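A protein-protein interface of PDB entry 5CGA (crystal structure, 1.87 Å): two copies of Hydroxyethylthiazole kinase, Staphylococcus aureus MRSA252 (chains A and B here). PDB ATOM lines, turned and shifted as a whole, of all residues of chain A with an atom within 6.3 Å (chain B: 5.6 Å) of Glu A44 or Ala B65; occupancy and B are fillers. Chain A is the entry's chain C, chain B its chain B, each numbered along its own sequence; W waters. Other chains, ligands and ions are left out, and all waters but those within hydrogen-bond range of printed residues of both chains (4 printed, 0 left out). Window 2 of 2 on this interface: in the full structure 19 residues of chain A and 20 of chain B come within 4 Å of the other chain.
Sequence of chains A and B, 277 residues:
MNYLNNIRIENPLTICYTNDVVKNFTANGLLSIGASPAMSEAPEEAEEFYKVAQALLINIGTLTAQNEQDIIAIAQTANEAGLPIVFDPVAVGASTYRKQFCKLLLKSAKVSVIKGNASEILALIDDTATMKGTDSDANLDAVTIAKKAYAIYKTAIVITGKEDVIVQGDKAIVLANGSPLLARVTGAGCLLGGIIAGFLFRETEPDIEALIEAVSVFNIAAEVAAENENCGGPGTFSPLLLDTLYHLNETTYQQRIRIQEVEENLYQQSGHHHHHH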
ATOM      1  N   GLU A  41     -33.282 -12.634  -4.195  1.00  0.00           N
ATOM      2  CA  GLU A  41     -34.256 -13.535  -4.715  1.00  0.00           C
ATOM      3  C   GLU A  41     -33.734 -14.635  -5.690  1.00  0.00           C
ATOM      4  O   GLU A  41     -34.528 -15.454  -6.159  1.00  0.00           O
ATOM      5  CB  GLU A  41     -35.367 -12.741  -5.395  1.00  0.00           C
ATOM      6  CG  GLU A  41     -36.093 -11.834  -4.426  1.00  0.00           C
ATOM      7  CD  GLU A  41     -37.301 -11.131  -5.044  1.00  0.00           C
ATOM      8  OE1 GLU A  41     -37.481 -11.212  -6.300  1.00  0.00           O
ATOM      9  OE2 GLU A  41     -38.067 -10.519  -4.252  1.00  0.00           O
ATOM     10  N   ALA A  42     -32.449 -14.580  -6.075  1.00  0.00           N
ATOM     11  CA  ALA A  42     -31.874 -15.456  -7.019  1.00  0.00           C
ATOM     12  C   ALA A  42     -31.414 -16.753  -6.319  1.00  0.00           C
ATOM     13  O   ALA A  42     -30.631 -16.683  -5.388  1.00  0.00           O
ATOM     14  CB  ALA A  42     -30.651 -14.816  -7.626  1.00  0.00           C
ATOM     15  N   PRO A  43     -31.965 -17.894  -6.718  1.00  0.00           N
ATOM     16  CA  PRO A  43     -31.541 -19.133  -6.089  1.00  0.00           C
ATOM     17  C   PRO A  43     -30.073 -19.389  -6.298  1.00  0.00           C
ATOM     18  O   PRO A  43     -29.478 -20.046  -5.488  1.00  0.00           O
ATOM     19  CB  PRO A  43     -32.372 -20.220  -6.821  1.00  0.00           C
ATOM     20  CG  PRO A  43     -33.641 -19.510  -7.166  1.00  0.00           C
ATOM     21  CD  PRO A  43     -33.146 -18.098  -7.578  1.00  0.00           C
ATOM     22  N   GLU A  44     -29.503 -18.826  -7.339  1.00  0.00           N
ATOM     23  CA  GLU A  44     -28.109 -18.990  -7.680  1.00  0.00           C
ATOM     24  C   GLU A  44     -27.166 -18.410  -6.640  1.00  0.00           C
ATOM     25  O   GLU A  44     -25.980 -18.768  -6.610  1.00  0.00           O
ATOM     26  CB  GLU A  44     -27.814 -18.296  -9.042  1.00  0.00           C
ATOM     27  CG  GLU A  44     -28.568 -18.925 -10.220  1.00  0.00           C
ATOM     28  CD  GLU A  44     -29.948 -18.328 -10.510  1.00  0.00           C
ATOM     29  OE1 GLU A  44     -30.568 -17.678  -9.622  1.00  0.00           O
ATOM     30  OE2 GLU A  44     -30.418 -18.501 -11.636  1.00  0.00           O
ATOM     31  N   GLU A  45     -27.629 -17.555  -5.764  1.00  0.00           N
ATOM     32  CA  GLU A  45     -26.738 -17.046  -4.739  1.00  0.00           C
ATOM     33  C   GLU A  45     -27.170 -17.397  -3.323  1.00  0.00           C
ATOM     34  O   GLU A  45     -26.627 -16.856  -2.356  1.00  0.00           O
ATOM     35  CB  GLU A  45     -26.582 -15.509  -4.855  1.00  0.00           C
ATOM     36  CG  GLU A  45     -27.785 -14.676  -4.581  1.00  0.00           C
ATOM     37  CD  GLU A  45     -27.600 -13.179  -4.906  1.00  0.00           C
ATOM     38  OE1 GLU A  45     -26.486 -12.761  -5.349  1.00  0.00           O
ATOM     39  OE2 GLU A  45     -28.557 -12.365  -4.678  1.00  0.00           O
ATOM     40  N   ALA A  46     -28.255 -18.174  -3.218  1.00  0.00           N
ATOM     41  CA  ALA A  46     -28.822 -18.469  -1.940  1.00  0.00           C
ATOM     42  C   ALA A  46     -27.832 -19.249  -1.056  1.00  0.00           C
ATOM     43  O   ALA A  46     -27.713 -18.939   0.120  1.00  0.00           O
ATOM     44  CB  ALA A  46     -30.096 -19.299  -2.101  1.00  0.00           C
ATOM     45  N   GLU A  47     -27.132 -20.210  -1.612  1.00  0.00           N
ATOM     46  CA  GLU A  47     -26.189 -20.980  -0.800  1.00  0.00           C
ATOM     47  C   GLU A  47     -25.091 -20.106  -0.160  1.00  0.00           C
ATOM     48  O   GLU A  47     -24.828 -20.172   1.064  1.00  0.00           O
ATOM     49  CB  GLU A  47     -25.619 -22.153  -1.598  1.00  0.00           C
ATOM     50  CG  GLU A  47     -25.113 -23.276  -0.708  1.00  0.00           C
ATOM     51  CD  GLU A  47     -24.408 -24.438  -1.439  1.00  0.00           C
ATOM     52  OE1 GLU A  47     -24.324 -24.372  -2.671  1.00  0.00           O
ATOM     53  N   GLU A  48     -24.476 -19.235  -0.951  1.00  0.00           N
ATOM     54  CA  GLU A  48     -23.483 -18.332  -0.436  1.00  0.00           C
ATOM     55  C   GLU A  48     -24.029 -17.312   0.552  1.00  0.00           C
ATOM     56  O   GLU A  48     -23.431 -17.071   1.577  1.00  0.00           O
ATOM     57  CB  GLU A  48     -22.737 -17.622  -1.597  1.00  0.00           C
ATOM     58  CG  GLU A  48     -21.846 -18.603  -2.312  1.00  0.00           C
ATOM     59  CD  GLU A  48     -21.090 -17.995  -3.491  1.00  0.00           C
ATOM     60  OE1 GLU A  48     -21.677 -17.246  -4.238  1.00  0.00           O
ATOM     61  OE2 GLU A  48     -19.953 -18.411  -3.725  1.00  0.00           O
ATOM     62  N   ASP A  70     -38.770 -20.881  -7.464  1.00  0.00           N
ATOM     63  CA  ASP A  70     -37.685 -20.247  -6.755  1.00  0.00           C
ATOM     64  C   ASP A  70     -37.844 -20.266  -5.222  1.00  0.00           C
ATOM     65  O   ASP A  70     -36.887 -20.490  -4.493  1.00  0.00           O
ATOM     66  CB  ASP A  70     -37.451 -18.817  -7.192  1.00  0.00           C
ATOM     67  CG  ASP A  70     -36.829 -18.717  -8.632  1.00  0.00           C
ATOM     68  OD1 ASP A  70     -36.528 -19.767  -9.217  1.00  0.00           O
ATOM     69  OD2 ASP A  70     -36.738 -17.591  -9.132  1.00  0.00           O
ATOM     70  N   LEU B  63     -30.487  -8.718  -8.745  1.00  0.00           N
ATOM     71  CA  LEU B  63     -30.244  -9.524  -9.896  1.00  0.00           C
ATOM     72  C   LEU B  63     -30.852 -10.892  -9.821  1.00  0.00           C
ATOM     73  O   LEU B  63     -30.651 -11.628  -8.845  1.00  0.00           O
ATOM     74  CB  LEU B  63     -28.708  -9.713 -10.081  1.00  0.00           C
ATOM     75  CG  LEU B  63     -28.235 -10.371 -11.315  1.00  0.00           C
ATOM     76  CD1 LEU B  63     -28.601  -9.557 -12.529  1.00  0.00           C
ATOM     77  CD2 LEU B  63     -26.736 -10.630 -11.224  1.00  0.00           C
ATOM     78  N   THR B  64     -31.538 -11.285 -10.869  1.00  0.00           N
ATOM     79  CA  THR B  64     -32.012 -12.661 -11.040  1.00  0.00           C
ATOM     80  C   THR B  64     -31.902 -13.082 -12.492  1.00  0.00           C
ATOM     81  O   THR B  64     -31.602 -12.262 -13.359  1.00  0.00           O
ATOM     82  CB  THR B  64     -33.502 -12.790 -10.623  1.00  0.00           C
ATOM     83  OG1 THR B  64     -34.327 -11.997 -11.475  1.00  0.00           O
ATOM     84  CG2 THR B  64     -33.755 -12.402  -9.146  1.00  0.00           C
ATOM     85  N   ALA B  65     -32.152 -14.345 -12.778  1.00  0.00           N
ATOM     86  CA  ALA B  65     -32.103 -14.897 -14.119  1.00  0.00           C
ATOM     87  C   ALA B  65     -33.049 -14.199 -15.122  1.00  0.00           C
ATOM     88  O   ALA B  65     -32.656 -13.982 -16.253  1.00  0.00           O
ATOM     89  CB  ALA B  65     -32.422 -16.367 -14.103  1.00  0.00           C
ATOM     90  N   GLN B  66     -34.176 -13.696 -14.651  1.00  0.00           N
ATOM     91  CA  GLN B  66     -35.078 -12.830 -15.448  1.00  0.00           C
ATOM     92  C   GLN B  66     -34.431 -11.526 -15.992  1.00  0.00           C
ATOM     93  O   GLN B  66     -34.843 -11.032 -17.027  1.00  0.00           O
ATOM     94  N   ASN B  67     -33.417 -11.003 -15.313  1.00  0.00           N
ATOM     95  CA  ASN B  67     -32.808  -9.741 -15.633  1.00  0.00           C
ATOM     96  C   ASN B  67     -31.520  -9.902 -16.502  1.00  0.00           C
ATOM     97  O   ASN B  67     -31.123  -8.912 -17.106  1.00  0.00           O
ATOM     98  CB  ASN B  67     -32.282  -9.033 -14.353  1.00  0.00           C
ATOM     99  CG  ASN B  67     -33.330  -8.679 -13.357  1.00  0.00           C
ATOM    100  OD1 ASN B  67     -33.122  -8.891 -12.171  1.00  0.00           O
ATOM    101  ND2 ASN B  67     -34.448  -8.118 -13.806  1.00  0.00           N
ATOM    102  N   GLU B  68     -30.810 -11.030 -16.420  1.00  0.00           N
ATOM    103  CA  GLU B  68     -29.409 -11.044 -16.821  1.00  0.00           C
ATOM    104  C   GLU B  68     -29.251 -10.688 -18.298  1.00  0.00           C
ATOM    105  O   GLU B  68     -28.478  -9.787 -18.612  1.00  0.00           O
ATOM    106  CB  GLU B  68     -28.740 -12.399 -16.578  1.00  0.00           C
ATOM    107  CG  GLU B  68     -28.547 -12.739 -15.113  1.00  0.00           C
ATOM    108  CD  GLU B  68     -28.209 -14.237 -14.974  1.00  0.00           C
ATOM    109  OE1 GLU B  68     -27.299 -14.711 -15.671  1.00  0.00           O
ATOM    110  OE2 GLU B  68     -28.829 -14.916 -14.134  1.00  0.00           O
ATOM    111  N   GLN B  69     -29.963 -11.402 -19.161  1.00  0.00           N
ATOM    112  CA  GLN B  69     -29.802 -11.152 -20.620  1.00  0.00           C
ATOM    113  C   GLN B  69     -30.339  -9.755 -20.943  1.00  0.00           C
ATOM    114  O   GLN B  69     -29.757  -9.083 -21.820  1.00  0.00           O
ATOM    115  CB  GLN B  69     -30.363 -12.219 -21.571  1.00  0.00           C
ATOM    116  CG  GLN B  69     -29.245 -12.926 -22.407  1.00  0.00           C
ATOM    117  CD  GLN B  69     -28.670 -12.088 -23.577  1.00  0.00           C
ATOM    118  OE1 GLN B  69     -28.650 -10.800 -23.658  1.00  0.00           O
ATOM    119  N   THR B  96     -20.596 -15.410  -6.032  1.00  0.00           N
ATOM    120  CA  THR B  96     -19.997 -15.717  -7.305  1.00  0.00           C
ATOM    121  C   THR B  96     -20.966 -15.407  -8.439  1.00  0.00           C
ATOM    122  O   THR B  96     -20.576 -14.945  -9.498  1.00  0.00           O
ATOM    123  CB  THR B  96     -19.465 -17.163  -7.373  1.00  0.00           C
ATOM    124  OG1 THR B  96     -20.557 -18.059  -7.347  1.00  0.00           O
ATOM    125  CG2 THR B  96     -18.629 -17.442  -6.170  1.00  0.00           C
ATOM    126  N   TYR B  97     -22.261 -15.604  -8.190  1.00  0.00           N
ATOM    127  CA  TYR B  97     -23.275 -15.257  -9.165  1.00  0.00           C
ATOM    128  C   TYR B  97     -23.116 -13.797  -9.572  1.00  0.00           C
ATOM    129  O   TYR B  97     -23.123 -13.476 -10.787  1.00  0.00           O
ATOM    130  CB  TYR B  97     -24.685 -15.510  -8.507  1.00  0.00           C
ATOM    131  CG  TYR B  97     -25.859 -15.131  -9.363  1.00  0.00           C
ATOM    132  CD1 TYR B  97     -26.063 -15.721 -10.621  1.00  0.00           C
ATOM    133  CD2 TYR B  97     -26.750 -14.168  -8.927  1.00  0.00           C
ATOM    134  CE1 TYR B  97     -27.173 -15.345 -11.404  1.00  0.00           C
ATOM    135  CE2 TYR B  97     -27.834 -13.778  -9.682  1.00  0.00           C
ATOM    136  CZ  TYR B  97     -28.036 -14.360 -10.951  1.00  0.00           C
ATOM    137  OH  TYR B  97     -29.130 -13.893 -11.634  1.00  0.00           O
HETATM  138  O   HOH W   1     -23.479 -17.507  -6.189  1.00  0.00           O
HETATM  139  O   HOH W   2     -28.949 -17.479 -14.023  1.00  0.00           O
HETATM  140  O   HOH W   3     -32.580 -15.958 -10.390  1.00  0.00           O
HETATM  141  O   HOH W   4     -30.888 -11.754  -6.105  1.00  0.00           O
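Water W2 bridges OE2 of Glu B68 (2.6 Å) and OE2 of Glu A44 (3.0 Å). Water W1 lies within hydrogen-bond range of OE1 of Glu A48 (2.7 Å), O of Glu A44 (2.8 Å), N of Tyr B97 (3.0 Å) and OG1 of Thr B96 (3.2 Å). Water W4 lies within hydrogen-bond range of the backbone carbonyl oxygen (O) of Leu B63 (2.8 Å), the side-chain carboxylate (OE2) of Glu A45 (2.8 Å), the backbone NH (N) of Glu A41 (3.2 Å) and the backbone NH (N) of Ala A42 (3.2 Å). Water W3 lies within hydrogen-bond range of OE1 of Glu A44 (2.8 Å) and N of Ala B65 (2.9 Å).
Among the printed residues, pairs that only touch across the chains: Ala A42 with Leu B63 (3.4 Å), Glu A44 with Tyr B97 (3.5 Å), Ala A42 with Tyr B97 (3.6 Å), Glu A44 with Ala B65 (3.8 Å), Glu A45 with Tyr B97 (3.9 Å) and Ala A42 with Thr B64 (3.99 Å).
The side-chain amide oxygen (OD1) of Asn B67 lies within hydrogen-bond range of the backbone NH (N) of Thr B64 (3.2 Å). O of Thr B64 lies close to OH of Tyr B97. OH of Tyr B97 lies within hydrogen-bond range of N of Ala B65 (3.3 Å). The side-chain carboxylate of Glu B68 is in hydrogen-bond range of the side-chain hydroxyl of Tyr B97 (2.7 Å).
The backbone NH (N) of Thr B96 lies within hydrogen-bond range of the side-chain carboxylate (OE1) of Glu A48, at 2.8 Å.
Hydrophobic or aromatic side chains of chain A that line the printed part of chain B: Ala A42. Printed residues of chain B that touch a printed residue of chain A: Leu B63, Thr B64, Ala B65, Thr B96 and Tyr B97. Among the printed residues, no Asp or Glu carboxylate lies within 4 Å of a Lys or Arg side-chain nitrogen of the other chain.
No position is printed for both chains. Of the 7 pairs that touch across the chains among the printed residues, none has its exchanged pair printed and touching as well.
Of chain B, only Ala B65 and Tyr B97 come within 4 Å of Glu A44. Printed residues of chain A within 4 Å of Leu B63: Ala A42 (3.4 Å). Printed residues of chain A within 4 Å of Tyr B97: Ala A42, Glu A44 and Glu A45. Glu A41 touches none of the printed residues of chain B. Asn B67 touches none of the printed residues of chain A. The nearest residue of chain A that does not touch Ala B65 is Ala A42 (5.4 Å).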
